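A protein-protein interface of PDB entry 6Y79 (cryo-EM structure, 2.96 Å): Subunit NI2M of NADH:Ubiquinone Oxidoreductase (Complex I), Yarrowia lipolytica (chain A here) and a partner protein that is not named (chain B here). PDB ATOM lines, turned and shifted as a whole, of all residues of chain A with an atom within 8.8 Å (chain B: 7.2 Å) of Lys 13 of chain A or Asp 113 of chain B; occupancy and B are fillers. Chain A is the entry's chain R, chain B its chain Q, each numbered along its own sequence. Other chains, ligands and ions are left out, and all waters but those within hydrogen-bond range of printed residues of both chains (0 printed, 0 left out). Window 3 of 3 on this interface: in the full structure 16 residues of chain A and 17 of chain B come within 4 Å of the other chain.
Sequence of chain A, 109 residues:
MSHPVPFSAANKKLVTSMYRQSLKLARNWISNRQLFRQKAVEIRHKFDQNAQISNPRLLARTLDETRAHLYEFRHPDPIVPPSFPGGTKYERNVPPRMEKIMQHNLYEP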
ATOM      1  N   SER A   8      26.490  40.405 -15.539  1.00  0.00           N
ATOM      2  CA  SER A   8      26.494  40.596 -16.982  1.00  0.00           C
ATOM      3  C   SER A   8      25.590  39.547 -17.588  1.00  0.00           C
ATOM      4  O   SER A   8      25.008  38.721 -16.883  1.00  0.00           O
ATOM      5  CB  SER A   8      27.882  40.462 -17.593  1.00  0.00           C
ATOM      6  OG  SER A   8      28.143  39.140 -17.975  1.00  0.00           O
ATOM      7  N   ALA A   9      25.498  39.574 -18.914  1.00  0.00           N
ATOM      8  CA  ALA A   9      24.855  38.467 -19.604  1.00  0.00           C
ATOM      9  C   ALA A   9      25.851  37.357 -19.924  1.00  0.00           C
ATOM     10  O   ALA A   9      25.472  36.180 -19.977  1.00  0.00           O
ATOM     11  CB  ALA A   9      24.176  38.969 -20.871  1.00  0.00           C
ATOM     12  N   ALA A  10      27.128  37.706 -20.120  1.00  0.00           N
ATOM     13  CA  ALA A  10      28.124  36.713 -20.524  1.00  0.00           C
ATOM     14  C   ALA A  10      28.630  35.914 -19.326  1.00  0.00           C
ATOM     15  O   ALA A  10      28.852  34.703 -19.416  1.00  0.00           O
ATOM     16  CB  ALA A  10      29.295  37.399 -21.224  1.00  0.00           C
ATOM     17  N   ASN A  11      28.821  36.576 -18.188  1.00  0.00           N
ATOM     18  CA  ASN A  11      29.148  35.856 -16.956  1.00  0.00           C
ATOM     19  C   ASN A  11      27.986  34.981 -16.513  1.00  0.00           C
ATOM     20  O   ASN A  11      28.195  33.875 -15.993  1.00  0.00           O
ATOM     21  CB  ASN A  11      29.529  36.839 -15.853  1.00  0.00           C
ATOM     22  CG  ASN A  11      29.867  36.165 -14.551  1.00  0.00           C
ATOM     23  OD1 ASN A  11      30.417  35.078 -14.520  1.00  0.00           O
ATOM     24  ND2 ASN A  11      29.478  36.803 -13.451  1.00  0.00           N
ATOM     25  N   LYS A  12      26.756  35.440 -16.769  1.00  0.00           N
ATOM     26  CA  LYS A  12      25.576  34.620 -16.524  1.00  0.00           C
ATOM     27  C   LYS A  12      25.568  33.391 -17.414  1.00  0.00           C
ATOM     28  O   LYS A  12      25.306  32.288 -16.938  1.00  0.00           O
ATOM     29  CB  LYS A  12      24.310  35.436 -16.750  1.00  0.00           C
ATOM     30  CG  LYS A  12      23.073  34.709 -16.320  1.00  0.00           C
ATOM     31  CD  LYS A  12      21.994  35.685 -15.942  1.00  0.00           C
ATOM     32  CE  LYS A  12      20.989  35.878 -17.056  1.00  0.00           C
ATOM     33  NZ  LYS A  12      19.738  36.528 -16.575  1.00  0.00           N
ATOM     34  N   LYS A  13      25.825  33.584 -18.717  1.00  0.00           N
ATOM     35  CA  LYS A  13      25.995  32.490 -19.675  1.00  0.00           C
ATOM     36  C   LYS A  13      26.978  31.443 -19.168  1.00  0.00           C
ATOM     37  O   LYS A  13      26.647  30.247 -19.087  1.00  0.00           O
ATOM     38  CB  LYS A  13      26.491  33.072 -20.998  1.00  0.00           C
ATOM     39  CG  LYS A  13      26.726  32.077 -22.106  1.00  0.00           C
ATOM     40  CD  LYS A  13      25.416  31.557 -22.620  1.00  0.00           C
ATOM     41  CE  LYS A  13      24.658  32.683 -23.298  1.00  0.00           C
ATOM     42  NZ  LYS A  13      23.359  32.230 -23.832  1.00  0.00           N
ATOM     43  N   LEU A  14      28.148  31.909 -18.721  1.00  0.00           N
ATOM     44  CA  LEU A  14      29.223  31.041 -18.255  1.00  0.00           C
ATOM     45  C   LEU A  14      28.800  30.203 -17.049  1.00  0.00           C
ATOM     46  O   LEU A  14      28.913  28.969 -17.072  1.00  0.00           O
ATOM     47  CB  LEU A  14      30.439  31.900 -17.915  1.00  0.00           C
ATOM     48  CG  LEU A  14      31.815  31.267 -17.775  1.00  0.00           C
ATOM     49  CD1 LEU A  14      32.838  32.218 -18.372  1.00  0.00           C
ATOM     50  CD2 LEU A  14      32.136  30.977 -16.321  1.00  0.00           C
ATOM     51  N   VAL A  15      28.272  30.837 -15.993  1.00  0.00           N
ATOM     52  CA  VAL A  15      28.023  30.032 -14.788  1.00  0.00           C
ATOM     53  C   VAL A  15      26.648  29.366 -14.783  1.00  0.00           C
ATOM     54  O   VAL A  15      26.429  28.436 -13.994  1.00  0.00           O
ATOM     55  CB  VAL A  15      28.244  30.821 -13.489  1.00  0.00           C
ATOM     56  CG1 VAL A  15      29.704  31.142 -13.336  1.00  0.00           C
ATOM     57  CG2 VAL A  15      27.367  32.072 -13.416  1.00  0.00           C
ATOM     58  N   THR A  16      25.715  29.773 -15.661  1.00  0.00           N
ATOM     59  CA  THR A  16      24.545  28.930 -15.889  1.00  0.00           C
ATOM     60  C   THR A  16      24.956  27.621 -16.525  1.00  0.00           C
ATOM     61  O   THR A  16      24.468  26.550 -16.135  1.00  0.00           O
ATOM     62  CB  THR A  16      23.502  29.609 -16.775  1.00  0.00           C
ATOM     63  OG1 THR A  16      24.089  30.114 -17.981  1.00  0.00           O
ATOM     64  CG2 THR A  16      22.722  30.698 -16.050  1.00  0.00           C
ATOM     65  N   SER A  17      25.875  27.683 -17.495  1.00  0.00           N
ATOM     66  CA  SER A  17      26.343  26.447 -18.108  1.00  0.00           C
ATOM     67  C   SER A  17      27.208  25.633 -17.148  1.00  0.00           C
ATOM     68  O   SER A  17      27.184  24.399 -17.180  1.00  0.00           O
ATOM     69  CB  SER A  17      27.087  26.762 -19.400  1.00  0.00           C
ATOM     70  OG  SER A  17      26.183  27.294 -20.347  1.00  0.00           O
ATOM     71  N   MET A  18      27.944  26.305 -16.258  1.00  0.00           N
ATOM     72  CA  MET A  18      28.722  25.579 -15.255  1.00  0.00           C
ATOM     73  C   MET A  18      27.825  24.887 -14.228  1.00  0.00           C
ATOM     74  O   MET A  18      28.140  23.777 -13.779  1.00  0.00           O
ATOM     75  CB  MET A  18      29.689  26.534 -14.564  1.00  0.00           C
ATOM     76  CG  MET A  18      30.663  25.869 -13.601  1.00  0.00           C
ATOM     77  SD  MET A  18      31.826  27.032 -12.868  1.00  0.00           S
ATOM     78  CE  MET A  18      32.808  27.471 -14.298  1.00  0.00           C
ATOM     79  N   TYR A  19      26.696  25.505 -13.869  1.00  0.00           N
ATOM     80  CA  TYR A  19      25.754  24.855 -12.963  1.00  0.00           C
ATOM     81  C   TYR A  19      25.036  23.685 -13.635  1.00  0.00           C
ATOM     82  O   TYR A  19      24.820  22.646 -12.990  1.00  0.00           O
ATOM     83  CB  TYR A  19      24.755  25.886 -12.437  1.00  0.00           C
ATOM     84  CG  TYR A  19      23.781  25.351 -11.413  1.00  0.00           C
ATOM     85  CD1 TYR A  19      24.219  24.820 -10.211  1.00  0.00           C
ATOM     86  CD2 TYR A  19      22.422  25.409 -11.641  1.00  0.00           C
ATOM     87  CE1 TYR A  19      23.321  24.342  -9.275  1.00  0.00           C
ATOM     88  CE2 TYR A  19      21.523  24.930 -10.725  1.00  0.00           C
ATOM     89  CZ  TYR A  19      21.970  24.406  -9.545  1.00  0.00           C
ATOM     90  OH  TYR A  19      21.040  23.944  -8.649  1.00  0.00           O
ATOM     91  N   ARG A  20      24.659  23.854 -14.919  1.00  0.00           N
ATOM     92  CA  ARG A  20      24.221  22.746 -15.775  1.00  0.00           C
ATOM     93  C   ARG A  20      25.194  21.585 -15.718  1.00  0.00           C
ATOM     94  O   ARG A  20      24.800  20.433 -15.497  1.00  0.00           O
ATOM     95  CB  ARG A  20      24.121  23.197 -17.234  1.00  0.00           C
ATOM     96  CG  ARG A  20      22.883  23.905 -17.634  1.00  0.00           C
ATOM     97  CD  ARG A  20      22.941  24.424 -19.026  1.00  0.00           C
ATOM     98  NE  ARG A  20      22.350  23.439 -19.907  1.00  0.00           N
ATOM     99  CZ  ARG A  20      23.046  22.581 -20.632  1.00  0.00           C
ATOM    100  NH1 ARG A  20      24.370  22.587 -20.587  1.00  0.00           N
ATOM    101  NH2 ARG A  20      22.412  21.721 -21.401  1.00  0.00           N
ATOM    102  N   GLN A  21      26.478  21.893 -15.903  1.00  0.00           N
ATOM    103  CA  GLN A  21      27.518  20.879 -16.009  1.00  0.00           C
ATOM    104  C   GLN A  21      27.697  20.129 -14.697  1.00  0.00           C
ATOM    105  O   GLN A  21      27.823  18.901 -14.690  1.00  0.00           O
ATOM    106  CB  GLN A  21      28.834  21.524 -16.419  1.00  0.00           C
ATOM    107  CG  GLN A  21      28.970  21.737 -17.895  1.00  0.00           C
ATOM    108  CD  GLN A  21      30.210  22.517 -18.231  1.00  0.00           C
ATOM    109  OE1 GLN A  21      31.106  22.667 -17.400  1.00  0.00           O
ATOM    110  NE2 GLN A  21      30.268  23.038 -19.442  1.00  0.00           N
ATOM    111  N   VAL B  92      16.316  28.733 -12.750  1.00  0.00           N
ATOM    112  CA  VAL B  92      15.937  28.494 -14.134  1.00  0.00           C
ATOM    113  C   VAL B  92      16.842  27.418 -14.727  1.00  0.00           C
ATOM    114  O   VAL B  92      16.409  26.601 -15.543  1.00  0.00           O
ATOM    115  CB  VAL B  92      15.946  29.813 -14.938  1.00  0.00           C
ATOM    116  CG1 VAL B  92      17.287  30.472 -14.956  1.00  0.00           C
ATOM    117  CG2 VAL B  92      15.487  29.609 -16.358  1.00  0.00           C
ATOM    118  N   VAL B  96      15.680  23.735 -15.879  1.00  0.00           N
ATOM    119  CA  VAL B  96      16.074  23.171 -17.177  1.00  0.00           C
ATOM    120  C   VAL B  96      16.604  21.743 -17.005  1.00  0.00           C
ATOM    121  O   VAL B  96      16.282  20.843 -17.794  1.00  0.00           O
ATOM    122  CB  VAL B  96      17.076  24.098 -17.904  1.00  0.00           C
ATOM    123  CG1 VAL B  96      17.800  23.370 -19.011  1.00  0.00           C
ATOM    124  CG2 VAL B  96      16.328  25.263 -18.521  1.00  0.00           C
ATOM    125  N   ILE B 107      20.011  18.371 -23.484  1.00  0.00           N
ATOM    126  CA  ILE B 107      20.028  19.722 -24.022  1.00  0.00           C
ATOM    127  C   ILE B 107      21.470  20.204 -24.022  1.00  0.00           C
ATOM    128  O   ILE B 107      22.158  20.054 -23.012  1.00  0.00           O
ATOM    129  CB  ILE B 107      19.145  20.678 -23.200  1.00  0.00           C
ATOM    130  CG1 ILE B 107      17.712  20.185 -23.192  1.00  0.00           C
ATOM    131  CG2 ILE B 107      19.121  22.039 -23.807  1.00  0.00           C
ATOM    132  CD1 ILE B 107      17.179  20.072 -24.561  1.00  0.00           C
ATOM    133  N   PRO B 108      21.977  20.749 -25.122  1.00  0.00           N
ATOM    134  CA  PRO B 108      23.265  21.443 -25.076  1.00  0.00           C
ATOM    135  C   PRO B 108      23.100  22.823 -24.458  1.00  0.00           C
ATOM    136  O   PRO B 108      21.993  23.334 -24.315  1.00  0.00           O
ATOM    137  CB  PRO B 108      23.668  21.538 -26.549  1.00  0.00           C
ATOM    138  CG  PRO B 108      22.375  21.579 -27.261  1.00  0.00           C
ATOM    139  CD  PRO B 108      21.419  20.715 -26.482  1.00  0.00           C
ATOM    140  N   ASP B 109      24.233  23.435 -24.105  1.00  0.00           N
ATOM    141  CA  ASP B 109      24.179  24.668 -23.327  1.00  0.00           C
ATOM    142  C   ASP B 109      23.638  25.856 -24.128  1.00  0.00           C
ATOM    143  O   ASP B 109      23.063  26.774 -23.534  1.00  0.00           O
ATOM    144  CB  ASP B 109      25.562  24.990 -22.755  1.00  0.00           C
ATOM    145  CG  ASP B 109      26.632  25.053 -23.819  1.00  0.00           C
ATOM    146  OD1 ASP B 109      26.368  24.645 -24.966  1.00  0.00           O
ATOM    147  OD2 ASP B 109      27.742  25.527 -23.502  1.00  0.00           O
ATOM    148  N   HIS B 110      23.792  25.859 -25.463  1.00  0.00           N
ATOM    149  CA  HIS B 110      23.344  27.009 -26.254  1.00  0.00           C
ATOM    150  C   HIS B 110      21.882  26.931 -26.663  1.00  0.00           C
ATOM    151  O   HIS B 110      21.401  27.822 -27.373  1.00  0.00           O
ATOM    152  CB  HIS B 110      24.202  27.219 -27.519  1.00  0.00           C
ATOM    153  CG  HIS B 110      24.612  25.973 -28.258  1.00  0.00           C
ATOM    154  ND1 HIS B 110      25.729  25.246 -27.908  1.00  0.00           N
ATOM    155  CD2 HIS B 110      24.122  25.388 -29.381  1.00  0.00           C
ATOM    156  CE1 HIS B 110      25.883  24.241 -28.751  1.00  0.00           C
ATOM    157  NE2 HIS B 110      24.922  24.306 -29.654  1.00  0.00           N
ATOM    158  N   ASP B 111      21.179  25.869 -26.287  1.00  0.00           N
ATOM    159  CA  ASP B 111      19.730  25.790 -26.449  1.00  0.00           C
ATOM    160  C   ASP B 111      18.983  25.677 -25.126  1.00  0.00           C
ATOM    161  O   ASP B 111      17.750  25.764 -25.118  1.00  0.00           O
ATOM    162  CB  ASP B 111      19.336  24.604 -27.352  1.00  0.00           C
ATOM    163  CG  ASP B 111      20.028  24.627 -28.708  1.00  0.00           C
ATOM    164  OD1 ASP B 111      20.321  25.735 -29.198  1.00  0.00           O
ATOM    165  OD2 ASP B 111      20.312  23.542 -29.267  1.00  0.00           O
ATOM    166  N   ALA B 112      19.696  25.491 -24.018  1.00  0.00           N
ATOM    167  CA  ALA B 112      19.062  25.584 -22.709  1.00  0.00           C
ATOM    168  C   ALA B 112      18.810  27.031 -22.324  1.00  0.00           C
ATOM    169  O   ALA B 112      17.806  27.336 -21.673  1.00  0.00           O
ATOM    170  CB  ALA B 112      19.931  24.917 -21.651  1.00  0.00           C
ATOM    171  N   ASP B 113      19.720  27.925 -22.726  1.00  0.00           N
ATOM    172  CA  ASP B 113      19.653  29.332 -22.354  1.00  0.00           C
ATOM    173  C   ASP B 113      18.427  30.041 -22.911  1.00  0.00           C
ATOM    174  O   ASP B 113      17.897  30.944 -22.255  1.00  0.00           O
ATOM    175  CB  ASP B 113      20.909  30.057 -22.839  1.00  0.00           C
ATOM    176  CG  ASP B 113      21.114  29.944 -24.347  1.00  0.00           C
ATOM    177  OD1 ASP B 113      20.419  29.145 -25.003  1.00  0.00           O
ATOM    178  OD2 ASP B 113      21.986  30.656 -24.882  1.00  0.00           O
ATOM    179  N   GLU B 114      17.966  29.649 -24.098  1.00  0.00           N
ATOM    180  CA  GLU B 114      17.008  30.485 -24.804  1.00  0.00           C
ATOM    181  C   GLU B 114      15.572  30.048 -24.559  1.00  0.00           C
ATOM    182  O   GLU B 114      14.646  30.733 -25.004  1.00  0.00           O
ATOM    183  CB  GLU B 114      17.343  30.519 -26.299  1.00  0.00           C
ATOM    184  CG  GLU B 114      16.896  29.334 -27.140  1.00  0.00           C
ATOM    185  CD  GLU B 114      17.395  29.446 -28.576  1.00  0.00           C
ATOM    186  OE1 GLU B 114      17.784  28.416 -29.164  1.00  0.00           O
ATOM    187  OE2 GLU B 114      17.412  30.576 -29.110  1.00  0.00           O
ATOM    188  N   ILE B 115      15.347  28.946 -23.846  1.00  0.00           N
ATOM    189  CA  ILE B 115      13.967  28.651 -23.487  1.00  0.00           C
ATOM    190  C   ILE B 115      13.669  29.382 -22.179  1.00  0.00           C
ATOM    191  O   ILE B 115      13.739  28.831 -21.077  1.00  0.00           O
ATOM    192  CB  ILE B 115      13.664  27.129 -23.465  1.00  0.00           C
ATOM    193  CG1 ILE B 115      14.602  26.274 -22.603  1.00  0.00           C
ATOM    194  CG2 ILE B 115      13.754  26.568 -24.873  1.00  0.00           C
ATOM    195  CD1 ILE B 115      14.028  24.894 -22.328  1.00  0.00           C
ATOM    196  N   LYS B 116      13.333  30.663 -22.302  1.00  0.00           N
ATOM    197  CA  LYS B 116      13.102  31.467 -21.111  1.00  0.00           C
ATOM    198  C   LYS B 116      11.615  31.569 -20.804  1.00  0.00           C
ATOM    199  O   LYS B 116      11.228  31.735 -19.640  1.00  0.00           O
ATOM    200  CB  LYS B 116      13.741  32.848 -21.277  1.00  0.00           C
ATOM    201  CG  LYS B 116      15.260  32.792 -21.373  1.00  0.00           C
ATOM    202  CD  LYS B 116      15.884  34.175 -21.338  1.00  0.00           C
ATOM    203  CE  LYS B 116      15.657  34.916 -22.644  1.00  0.00           C
ATOM    204  NZ  LYS B 116      16.285  34.205 -23.787  1.00  0.00           N
ATOM    205  N   THR B 117      10.771  31.455 -21.824  1.00  0.00           N
ATOM    206  CA  THR B 117       9.339  31.345 -21.615  1.00  0.00           C
ATOM    207  C   THR B 117       8.960  29.888 -21.446  1.00  0.00           C
ATOM    208  O   THR B 117       9.754  28.988 -21.719  1.00  0.00           O
ATOM    209  CB  THR B 117       8.566  31.944 -22.782  1.00  0.00           C
ATOM    210  OG1 THR B 117       8.399  30.968 -23.802  1.00  0.00           O
ATOM    211  CG2 THR B 117       9.318  33.122 -23.354  1.00  0.00           C
ATOM    212  N   GLN B 120       8.128  28.662 -25.328  1.00  0.00           N
ATOM    213  CA  GLN B 120       9.330  28.278 -26.065  1.00  0.00           C
ATOM    214  C   GLN B 120       9.839  26.921 -25.602  1.00  0.00           C
ATOM    215  O   GLN B 120      10.287  26.111 -26.420  1.00  0.00           O
ATOM    216  CB  GLN B 120      10.421  29.332 -25.889  1.00  0.00           C
ATOM    217  CG  GLN B 120      10.206  30.612 -26.660  1.00  0.00           C
ATOM    218  CD  GLN B 120      11.109  31.721 -26.172  1.00  0.00           C
ATOM    219  OE1 GLN B 120      11.901  31.519 -25.258  1.00  0.00           O
ATOM    220  NE2 GLN B 120      10.971  32.909 -26.754  1.00  0.00           N
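Asp 109 of chain B touches Ser 17 of chain A (CB to OG, 3.4 Å).
CA of Asp 109 of chain B touches NH1 of Arg 20 of chain A, 3.4 Å away.
NE of Arg 20 of chain A touches CB of Ala 112 of chain B (3.3 Å).
Of the printed residues of chain B, Ser 17 of chain A touches Asp 109 (3.4 Å).
Printed residues of chain A within 4 Å of Pro 108 of chain B: Arg 20 (3.3 Å).
Printed residues of chain A within 4 Å of Asp 109 of chain B: Ser 17 (3.4 Å) and Arg 20 (3.4 Å).
Ala 112 of chain B touches just one residue of chain A: Arg 20.
Asp 113 of chain B touches just one residue of chain A: Lys 13.
The nearest residue of chain B that does not touch Lys 13 of chain A is Asp 109 of chain B (5.4 Å).
The nearest residue of chain A that does not touch Asp 113 of chain B is Thr 16 of chain A (5.8 Å).
ND1 of His 110 of chain B is in hydrogen-bond range of OD1 of Asp 109 of chain B (3.1 Å).
O of Lys 13 of chain A lies within hydrogen-bond range of OG1 of Thr 16 of chain A, at 2.8 Å.
The side-chain hydroxyl (OG) of Ser 17 of chain A sits at hydrogen-bond distance from the backbone carbonyl oxygen (O) of Lys 13 of chain A (3.2 Å).
The guanidinium group of Arg 20 of chain A lies close to the backbone carbonyl oxygen of Pro 108 of chain B (3.4 Å).
OD2 of Asp 113 of chain B lies close to NZ of Lys 13 of chain A, 2.3 Å away.
The backbone carbonyl oxygen (O) of Ile 107 of chain B sits close to the guanidinium group (NH2) of Arg 20 of chain A.
Printed residues of chain B that touch a printed residue of chain A: Ile 107, Pro 108, Asp 109, Ala 112 and Asp 113.
Printed residues of chain A that touch a printed residue of chain B: Lys 13, Ser 17 and Arg 20.
Among the printed residues, Asp or Glu carboxylates within 4 Å of a Lys or Arg side-chain nitrogen of the other chain: Lys 13 of chain A with Asp 113 of chain B (2.3 Å).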
